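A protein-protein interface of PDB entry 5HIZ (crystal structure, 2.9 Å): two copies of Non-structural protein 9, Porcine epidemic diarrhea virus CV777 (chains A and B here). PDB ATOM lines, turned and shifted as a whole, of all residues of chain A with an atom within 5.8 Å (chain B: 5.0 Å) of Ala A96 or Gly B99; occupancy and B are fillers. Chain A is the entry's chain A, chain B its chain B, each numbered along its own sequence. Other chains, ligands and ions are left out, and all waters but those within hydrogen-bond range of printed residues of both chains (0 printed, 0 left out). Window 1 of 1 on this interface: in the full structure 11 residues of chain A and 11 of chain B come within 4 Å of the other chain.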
ATOM      1  N   GLY A   7     -13.328 -15.009  -2.455  1.00  0.00           N
ATOM      2  CA  GLY A   7     -14.111 -15.887  -1.529  1.00  0.00           C
ATOM      3  C   GLY A   7     -15.346 -15.244  -0.910  1.00  0.00           C
ATOM      4  O   GLY A   7     -15.901 -15.771   0.077  1.00  0.00           O
ATOM      5  N   LEU A   9     -19.082 -14.499  -1.608  1.00  0.00           N
ATOM      6  CA  LEU A   9     -19.893 -15.335  -2.509  1.00  0.00           C
ATOM      7  C   LEU A   9     -21.386 -15.214  -2.330  1.00  0.00           C
ATOM      8  O   LEU A   9     -21.865 -15.067  -1.210  1.00  0.00           O
ATOM      9  CB  LEU A   9     -19.522 -16.801  -2.297  1.00  0.00           C
ATOM     10  CG  LEU A   9     -19.617 -17.812  -3.435  1.00  0.00           C
ATOM     11  CD1 LEU A   9     -18.482 -17.605  -4.392  1.00  0.00           C
ATOM     12  CD2 LEU A   9     -19.535 -19.199  -2.847  1.00  0.00           C
ATOM     13  N   TYR A  39     -20.975 -21.764  -8.912  1.00  0.00           N
ATOM     14  CA  TYR A  39     -20.035 -22.641  -8.218  1.00  0.00           C
ATOM     15  C   TYR A  39     -20.617 -23.996  -7.763  1.00  0.00           C
ATOM     16  O   TYR A  39     -20.034 -25.042  -8.055  1.00  0.00           O
ATOM     17  CB  TYR A  39     -19.337 -21.899  -7.047  1.00  0.00           C
ATOM     18  CG  TYR A  39     -18.177 -20.944  -7.420  1.00  0.00           C
ATOM     19  CD1 TYR A  39     -17.770 -20.766  -8.748  1.00  0.00           C
ATOM     20  CD2 TYR A  39     -17.477 -20.243  -6.431  1.00  0.00           C
ATOM     21  CE1 TYR A  39     -16.726 -19.903  -9.079  1.00  0.00           C
ATOM     22  CE2 TYR A  39     -16.420 -19.376  -6.756  1.00  0.00           C
ATOM     23  CZ  TYR A  39     -16.050 -19.214  -8.088  1.00  0.00           C
ATOM     24  OH  TYR A  39     -15.005 -18.373  -8.447  1.00  0.00           O
ATOM     25  N   THR A  91     -10.065 -27.173  -7.607  1.00  0.00           N
ATOM     26  CA  THR A  91     -10.112 -27.599  -6.201  1.00  0.00           C
ATOM     27  C   THR A  91     -10.228 -26.380  -5.339  1.00  0.00           C
ATOM     28  O   THR A  91     -10.979 -26.370  -4.362  1.00  0.00           O
ATOM     29  CB  THR A  91      -8.872 -28.361  -5.820  1.00  0.00           C
ATOM     30  OG1 THR A  91      -8.003 -28.295  -6.935  1.00  0.00           O
ATOM     31  CG2 THR A  91      -9.145 -29.845  -5.613  1.00  0.00           C
ATOM     32  N   LEU A  92      -9.518 -25.327  -5.741  1.00  0.00           N
ATOM     33  CA  LEU A  92      -9.530 -24.067  -5.011  1.00  0.00           C
ATOM     34  C   LEU A  92     -10.953 -23.578  -4.730  1.00  0.00           C
ATOM     35  O   LEU A  92     -11.349 -23.467  -3.578  1.00  0.00           O
ATOM     36  CB  LEU A  92      -8.717 -23.058  -5.803  1.00  0.00           C
ATOM     37  CG  LEU A  92      -8.441 -21.596  -5.428  1.00  0.00           C
ATOM     38  CD1 LEU A  92      -7.699 -21.468  -4.108  1.00  0.00           C
ATOM     39  CD2 LEU A  92      -7.675 -20.868  -6.605  1.00  0.00           C
ATOM     40  N   ARG A  93     -11.742 -23.335  -5.780  1.00  0.00           N
ATOM     41  CA  ARG A  93     -13.148 -22.929  -5.609  1.00  0.00           C
ATOM     42  C   ARG A  93     -13.997 -24.002  -4.913  1.00  0.00           C
ATOM     43  O   ARG A  93     -14.830 -23.670  -4.064  1.00  0.00           O
ATOM     44  CB  ARG A  93     -13.760 -22.519  -6.932  1.00  0.00           C
ATOM     45  CG  ARG A  93     -13.277 -21.148  -7.454  1.00  0.00           C
ATOM     46  CD  ARG A  93     -11.936 -21.208  -8.266  1.00  0.00           C
ATOM     47  NE  ARG A  93     -12.119 -21.163  -9.734  1.00  0.00           N
ATOM     48  CZ  ARG A  93     -12.070 -20.042 -10.470  1.00  0.00           C
ATOM     49  NH1 ARG A  93     -12.253 -20.086 -11.797  1.00  0.00           N
ATOM     50  NH2 ARG A  93     -11.840 -18.868  -9.870  1.00  0.00           N
ATOM     51  N   ARG A  94     -13.780 -25.283  -5.222  1.00  0.00           N
ATOM     52  CA  ARG A  94     -14.409 -26.323  -4.417  1.00  0.00           C
ATOM     53  C   ARG A  94     -14.252 -25.912  -2.939  1.00  0.00           C
ATOM     54  O   ARG A  94     -15.233 -25.590  -2.236  1.00  0.00           O
ATOM     55  CB  ARG A  94     -13.739 -27.669  -4.629  1.00  0.00           C
ATOM     56  CG  ARG A  94     -13.970 -28.283  -5.976  1.00  0.00           C
ATOM     57  CD  ARG A  94     -13.303 -29.678  -6.087  1.00  0.00           C
ATOM     58  NE  ARG A  94     -14.315 -30.660  -6.453  1.00  0.00           N
ATOM     59  CZ  ARG A  94     -14.816 -30.812  -7.674  1.00  0.00           C
ATOM     60  NH1 ARG A  94     -14.378 -30.082  -8.699  1.00  0.00           N
ATOM     61  NH2 ARG A  94     -15.777 -31.704  -7.868  1.00  0.00           N
ATOM     62  N   GLY A  95     -12.990 -25.878  -2.490  1.00  0.00           N
ATOM     63  CA  GLY A  95     -12.639 -25.424  -1.154  1.00  0.00           C
ATOM     64  C   GLY A  95     -13.448 -24.209  -0.750  1.00  0.00           C
ATOM     65  O   GLY A  95     -14.157 -24.232   0.292  1.00  0.00           O
ATOM     66  N   ALA A  96     -13.382 -23.150  -1.566  1.00  0.00           N
ATOM     67  CA  ALA A  96     -14.095 -21.920  -1.219  1.00  0.00           C
ATOM     68  C   ALA A  96     -15.557 -22.236  -0.780  1.00  0.00           C
ATOM     69  O   ALA A  96     -16.036 -21.741   0.276  1.00  0.00           O
ATOM     70  CB  ALA A  96     -14.040 -20.943  -2.378  1.00  0.00           C
ATOM     71  N   VAL A  97     -16.209 -23.122  -1.560  1.00  0.00           N
ATOM     72  CA  VAL A  97     -17.578 -23.545  -1.287  1.00  0.00           C
ATOM     73  C   VAL A  97     -17.685 -24.046   0.141  1.00  0.00           C
ATOM     74  O   VAL A  97     -18.163 -23.324   1.010  1.00  0.00           O
ATOM     75  CB  VAL A  97     -18.064 -24.633  -2.258  1.00  0.00           C
ATOM     76  CG1 VAL A  97     -19.546 -24.799  -2.138  1.00  0.00           C
ATOM     77  CG2 VAL A  97     -17.731 -24.279  -3.688  1.00  0.00           C
ATOM     78  N   LEU A  98     -17.218 -25.270   0.376  1.00  0.00           N
ATOM     79  CA  LEU A  98     -17.089 -25.846   1.718  1.00  0.00           C
ATOM     80  C   LEU A  98     -16.832 -24.808   2.769  1.00  0.00           C
ATOM     81  O   LEU A  98     -17.540 -24.755   3.769  1.00  0.00           O
ATOM     82  CB  LEU A  98     -15.917 -26.792   1.745  1.00  0.00           C
ATOM     83  CG  LEU A  98     -16.187 -27.806   0.662  1.00  0.00           C
ATOM     84  CD1 LEU A  98     -14.973 -28.630   0.363  1.00  0.00           C
ATOM     85  CD2 LEU A  98     -17.352 -28.682   1.124  1.00  0.00           C
ATOM     86  N   GLY A  99     -15.808 -23.991   2.537  1.00  0.00           N
ATOM     87  CA  GLY A  99     -15.485 -22.900   3.424  1.00  0.00           C
ATOM     88  C   GLY A  99     -16.726 -22.113   3.790  1.00  0.00           C
ATOM     89  O   GLY A  99     -17.138 -22.096   4.967  1.00  0.00           O
ATOM     90  N   TYR A 100     -17.326 -21.474   2.789  1.00  0.00           N
ATOM     91  CA  TYR A 100     -18.581 -20.765   3.000  1.00  0.00           C
ATOM     92  C   TYR A 100     -19.687 -21.662   3.615  1.00  0.00           C
ATOM     93  O   TYR A 100     -20.305 -21.284   4.599  1.00  0.00           O
ATOM     94  CB  TYR A 100     -19.015 -20.123   1.692  1.00  0.00           C
ATOM     95  CG  TYR A 100     -20.432 -19.591   1.631  1.00  0.00           C
ATOM     96  CD1 TYR A 100     -21.482 -20.253   2.268  1.00  0.00           C
ATOM     97  CD2 TYR A 100     -20.737 -18.447   0.869  1.00  0.00           C
ATOM     98  CE1 TYR A 100     -22.804 -19.776   2.201  1.00  0.00           C
ATOM     99  CE2 TYR A 100     -22.054 -17.954   0.781  1.00  0.00           C
ATOM    100  CZ  TYR A 100     -23.088 -18.636   1.450  1.00  0.00           C
ATOM    101  OH  TYR A 100     -24.407 -18.201   1.376  1.00  0.00           O
ATOM    102  N   ILE A 101     -19.925 -22.840   3.048  1.00  0.00           N
ATOM    103  CA  ILE A 101     -21.000 -23.718   3.535  1.00  0.00           C
ATOM    104  C   ILE A 101     -21.029 -23.799   5.057  1.00  0.00           C
ATOM    105  O   ILE A 101     -21.864 -23.152   5.693  1.00  0.00           O
ATOM    106  CB  ILE A 101     -20.887 -25.185   3.009  1.00  0.00           C
ATOM    107  CG1 ILE A 101     -20.784 -25.262   1.475  1.00  0.00           C
ATOM    108  CG2 ILE A 101     -22.018 -26.057   3.591  1.00  0.00           C
ATOM    109  CD1 ILE A 101     -21.808 -24.464   0.743  1.00  0.00           C
ATOM    110  N   ALA A 103     -19.679 -22.394   7.127  1.00  0.00           N
ATOM    111  CA  ALA A 103     -19.652 -21.027   7.700  1.00  0.00           C
ATOM    112  C   ALA A 103     -21.032 -20.380   7.875  1.00  0.00           C
ATOM    113  O   ALA A 103     -21.111 -19.319   8.491  1.00  0.00           O
ATOM    114  CB  ALA A 103     -18.728 -20.074   6.877  1.00  0.00           C
ATOM    115  N   GLY B  95      -8.478 -22.775  -0.322  1.00  0.00           N
ATOM    116  CA  GLY B  95      -9.804 -22.292  -0.733  1.00  0.00           C
ATOM    117  C   GLY B  95     -10.791 -22.190   0.417  1.00  0.00           C
ATOM    118  O   GLY B  95     -11.526 -21.191   0.532  1.00  0.00           O
ATOM    119  N   ALA B  96     -10.801 -23.205   1.286  1.00  0.00           N
ATOM    120  CA  ALA B  96     -11.690 -23.183   2.443  1.00  0.00           C
ATOM    121  C   ALA B  96     -11.525 -21.870   3.269  1.00  0.00           C
ATOM    122  O   ALA B  96     -12.529 -21.224   3.658  1.00  0.00           O
ATOM    123  CB  ALA B  96     -11.456 -24.420   3.290  1.00  0.00           C
ATOM    124  N   VAL B  97     -10.264 -21.469   3.490  1.00  0.00           N
ATOM    125  CA  VAL B  97      -9.941 -20.269   4.255  1.00  0.00           C
ATOM    126  C   VAL B  97     -10.653 -19.105   3.617  1.00  0.00           C
ATOM    127  O   VAL B  97     -11.575 -18.556   4.198  1.00  0.00           O
ATOM    128  CB  VAL B  97      -8.410 -19.979   4.307  1.00  0.00           C
ATOM    129  CG1 VAL B  97      -8.112 -18.699   5.091  1.00  0.00           C
ATOM    130  CG2 VAL B  97      -7.663 -21.138   4.919  1.00  0.00           C
ATOM    131  N   LEU B  98     -10.242 -18.754   2.404  1.00  0.00           N
ATOM    132  CA  LEU B  98     -10.890 -17.709   1.615  1.00  0.00           C
ATOM    133  C   LEU B  98     -12.410 -17.787   1.637  1.00  0.00           C
ATOM    134  O   LEU B  98     -13.075 -16.763   1.583  1.00  0.00           O
ATOM    135  CB  LEU B  98     -10.420 -17.804   0.182  1.00  0.00           C
ATOM    136  CG  LEU B  98      -8.906 -17.716   0.102  1.00  0.00           C
ATOM    137  CD1 LEU B  98      -8.361 -18.627  -0.948  1.00  0.00           C
ATOM    138  CD2 LEU B  98      -8.486 -16.272  -0.147  1.00  0.00           C
ATOM    139  N   GLY B  99     -12.952 -19.000   1.706  1.00  0.00           N
ATOM    140  CA  GLY B  99     -14.395 -19.200   1.836  1.00  0.00           C
ATOM    141  C   GLY B  99     -14.938 -18.649   3.137  1.00  0.00           C
ATOM    142  O   GLY B  99     -15.770 -17.740   3.138  1.00  0.00           O
ATOM    143  N   TYR B 100     -14.469 -19.207   4.245  1.00  0.00           N
ATOM    144  CA  TYR B 100     -14.626 -18.601   5.556  1.00  0.00           C
ATOM    145  C   TYR B 100     -14.363 -17.080   5.513  1.00  0.00           C
ATOM    146  O   TYR B 100     -15.228 -16.304   5.908  1.00  0.00           O
ATOM    147  CB  TYR B 100     -13.636 -19.287   6.451  1.00  0.00           C
ATOM    148  CG  TYR B 100     -13.819 -19.179   7.932  1.00  0.00           C
ATOM    149  CD1 TYR B 100     -13.319 -18.082   8.642  1.00  0.00           C
ATOM    150  CD2 TYR B 100     -14.388 -20.236   8.663  1.00  0.00           C
ATOM    151  CE1 TYR B 100     -13.429 -18.001  10.053  1.00  0.00           C
ATOM    152  CE2 TYR B 100     -14.510 -20.175  10.087  1.00  0.00           C
ATOM    153  CZ  TYR B 100     -14.021 -19.049  10.771  1.00  0.00           C
ATOM    154  OH  TYR B 100     -14.125 -18.970  12.160  1.00  0.00           O
ATOM    155  N   ILE B 101     -13.197 -16.658   5.007  1.00  0.00           N
ATOM    156  CA  ILE B 101     -12.783 -15.238   4.990  1.00  0.00           C
ATOM    157  C   ILE B 101     -13.921 -14.296   4.582  1.00  0.00           C
ATOM    158  O   ILE B 101     -14.455 -13.553   5.404  1.00  0.00           O
ATOM    159  CB  ILE B 101     -11.586 -14.959   4.004  1.00  0.00           C
ATOM    160  CG1 ILE B 101     -10.274 -15.670   4.408  1.00  0.00           C
ATOM    161  CG2 ILE B 101     -11.419 -13.419   3.736  1.00  0.00           C
ATOM    162  CD1 ILE B 101     -10.011 -15.718   5.853  1.00  0.00           C
ATOM    163  N   GLY B 102     -14.270 -14.331   3.297  1.00  0.00           N
ATOM    164  CA  GLY B 102     -15.329 -13.496   2.731  1.00  0.00           C
ATOM    165  C   GLY B 102     -16.732 -13.821   3.235  1.00  0.00           C
ATOM    166  O   GLY B 102     -17.658 -13.055   2.992  1.00  0.00           O
ATOM    167  N   ALA B 103     -16.889 -14.959   3.923  1.00  0.00           N
ATOM    168  CA  ALA B 103     -18.147 -15.289   4.636  1.00  0.00           C
ATOM    169  C   ALA B 103     -18.362 -14.390   5.863  1.00  0.00           C
ATOM    170  O   ALA B 103     -19.467 -13.856   6.057  1.00  0.00           O
ATOM    171  CB  ALA B 103     -18.203 -16.777   5.056  1.00  0.00           C
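Of the 15 printed residues of chain A, 7 touch a printed residue of chain B. Printed residues of chain A that touch a printed residue of chain B: Gly A7, Leu A92, Gly A95, Ala A96, Gly A99, Tyr A100 and Ala A103. Hydrophobic or aromatic side chains of chain A that line the printed part of chain B: Ala A96 and Ala A103. Along chain A the printed residues that touch a printed residue of chain B span positions 7 to 103. Of the 9 printed residues of chain B, 7 touch a printed residue of chain A. Printed residues of chain B that touch a printed residue of chain A: Gly B95, Ala B96, Leu B98, Gly B99, Tyr B100, Gly B102 and Ala B103. Hydrophobic or aromatic side chains of chain B within 4 Å of the printed part of chain A: Ala B103. Among the printed residues, 15 pairs touch across the chains. Among the printed residues, no Asp or Glu carboxylate lies within 4 Å of a Lys or Arg side-chain nitrogen of the other chain.
Of chain B, only Gly B95 (3.2 Å), Ala B96 (3.8 Å) and Gly B99 (3.4 Å) come within 4 Å of Ala A96. Gly B99 touches just these residues of chain A: Gly A7 (3.6 Å), Ala A96 (3.4 Å), Gly A99 (3.95 Å) and Tyr A100 (3.7 Å). Of the printed residues of chain B, Tyr A100 touches Gly B99 and Tyr B100. Printed residues of chain A within 4 Å of Tyr B100: Gly A99 (3.7 Å) and Tyr A100 (3.9 Å). Printed residues of chain B within 4 Å of Ala A103: Ala B103 (3.8 Å). Of the printed residues of chain B, Gly A99 touches Ala B96, Gly B99 and Tyr B100. The nearest printed residue of chain B that does not touch Gly A7 is Ala B103 (4.1 Å).
The backbone carbonyl oxygen of Gly A7 sits close to the backbone carbonyl oxygen of Leu B98 (3.4 Å). The backbone carbonyl oxygen (O) of Gly B95 lies close to the backbone NH (N) of Ala A96, 3.4 Å away.
Among the printed residues, merely in contact across the chains: Gly A7 with Gly B99 (3.6 Å), Gly A7 with Gly B102 (3.5 Å), Leu A92 with Gly B95 (3.4 Å), Gly A95 with Gly B95 (3.5 Å), Gly A95 with Ala B96 (3.4 Å), Ala A96 with Ala B96 (3.8 Å), Ala A96 with Gly B99 (3.4 Å), Gly A99 with Ala B96 (3.4 Å), Gly A99 with Gly B99 (3.95 Å), Gly A99 with Tyr B100 (3.7 Å), Tyr A100 with Gly B99 (3.7 Å), Tyr A100 with Tyr B100 (3.9 Å) and Ala A103 with Ala B103 (3.8 Å).
Gly A95 touches Ala B96, and with the chains exchanged Ala A96 touches Gly B95. Ala A96 touches its own counterpart, Ala B96. Gly B99 touches its own counterpart, Gly A99. Tyr B100 touches its own counterpart, Tyr A100.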
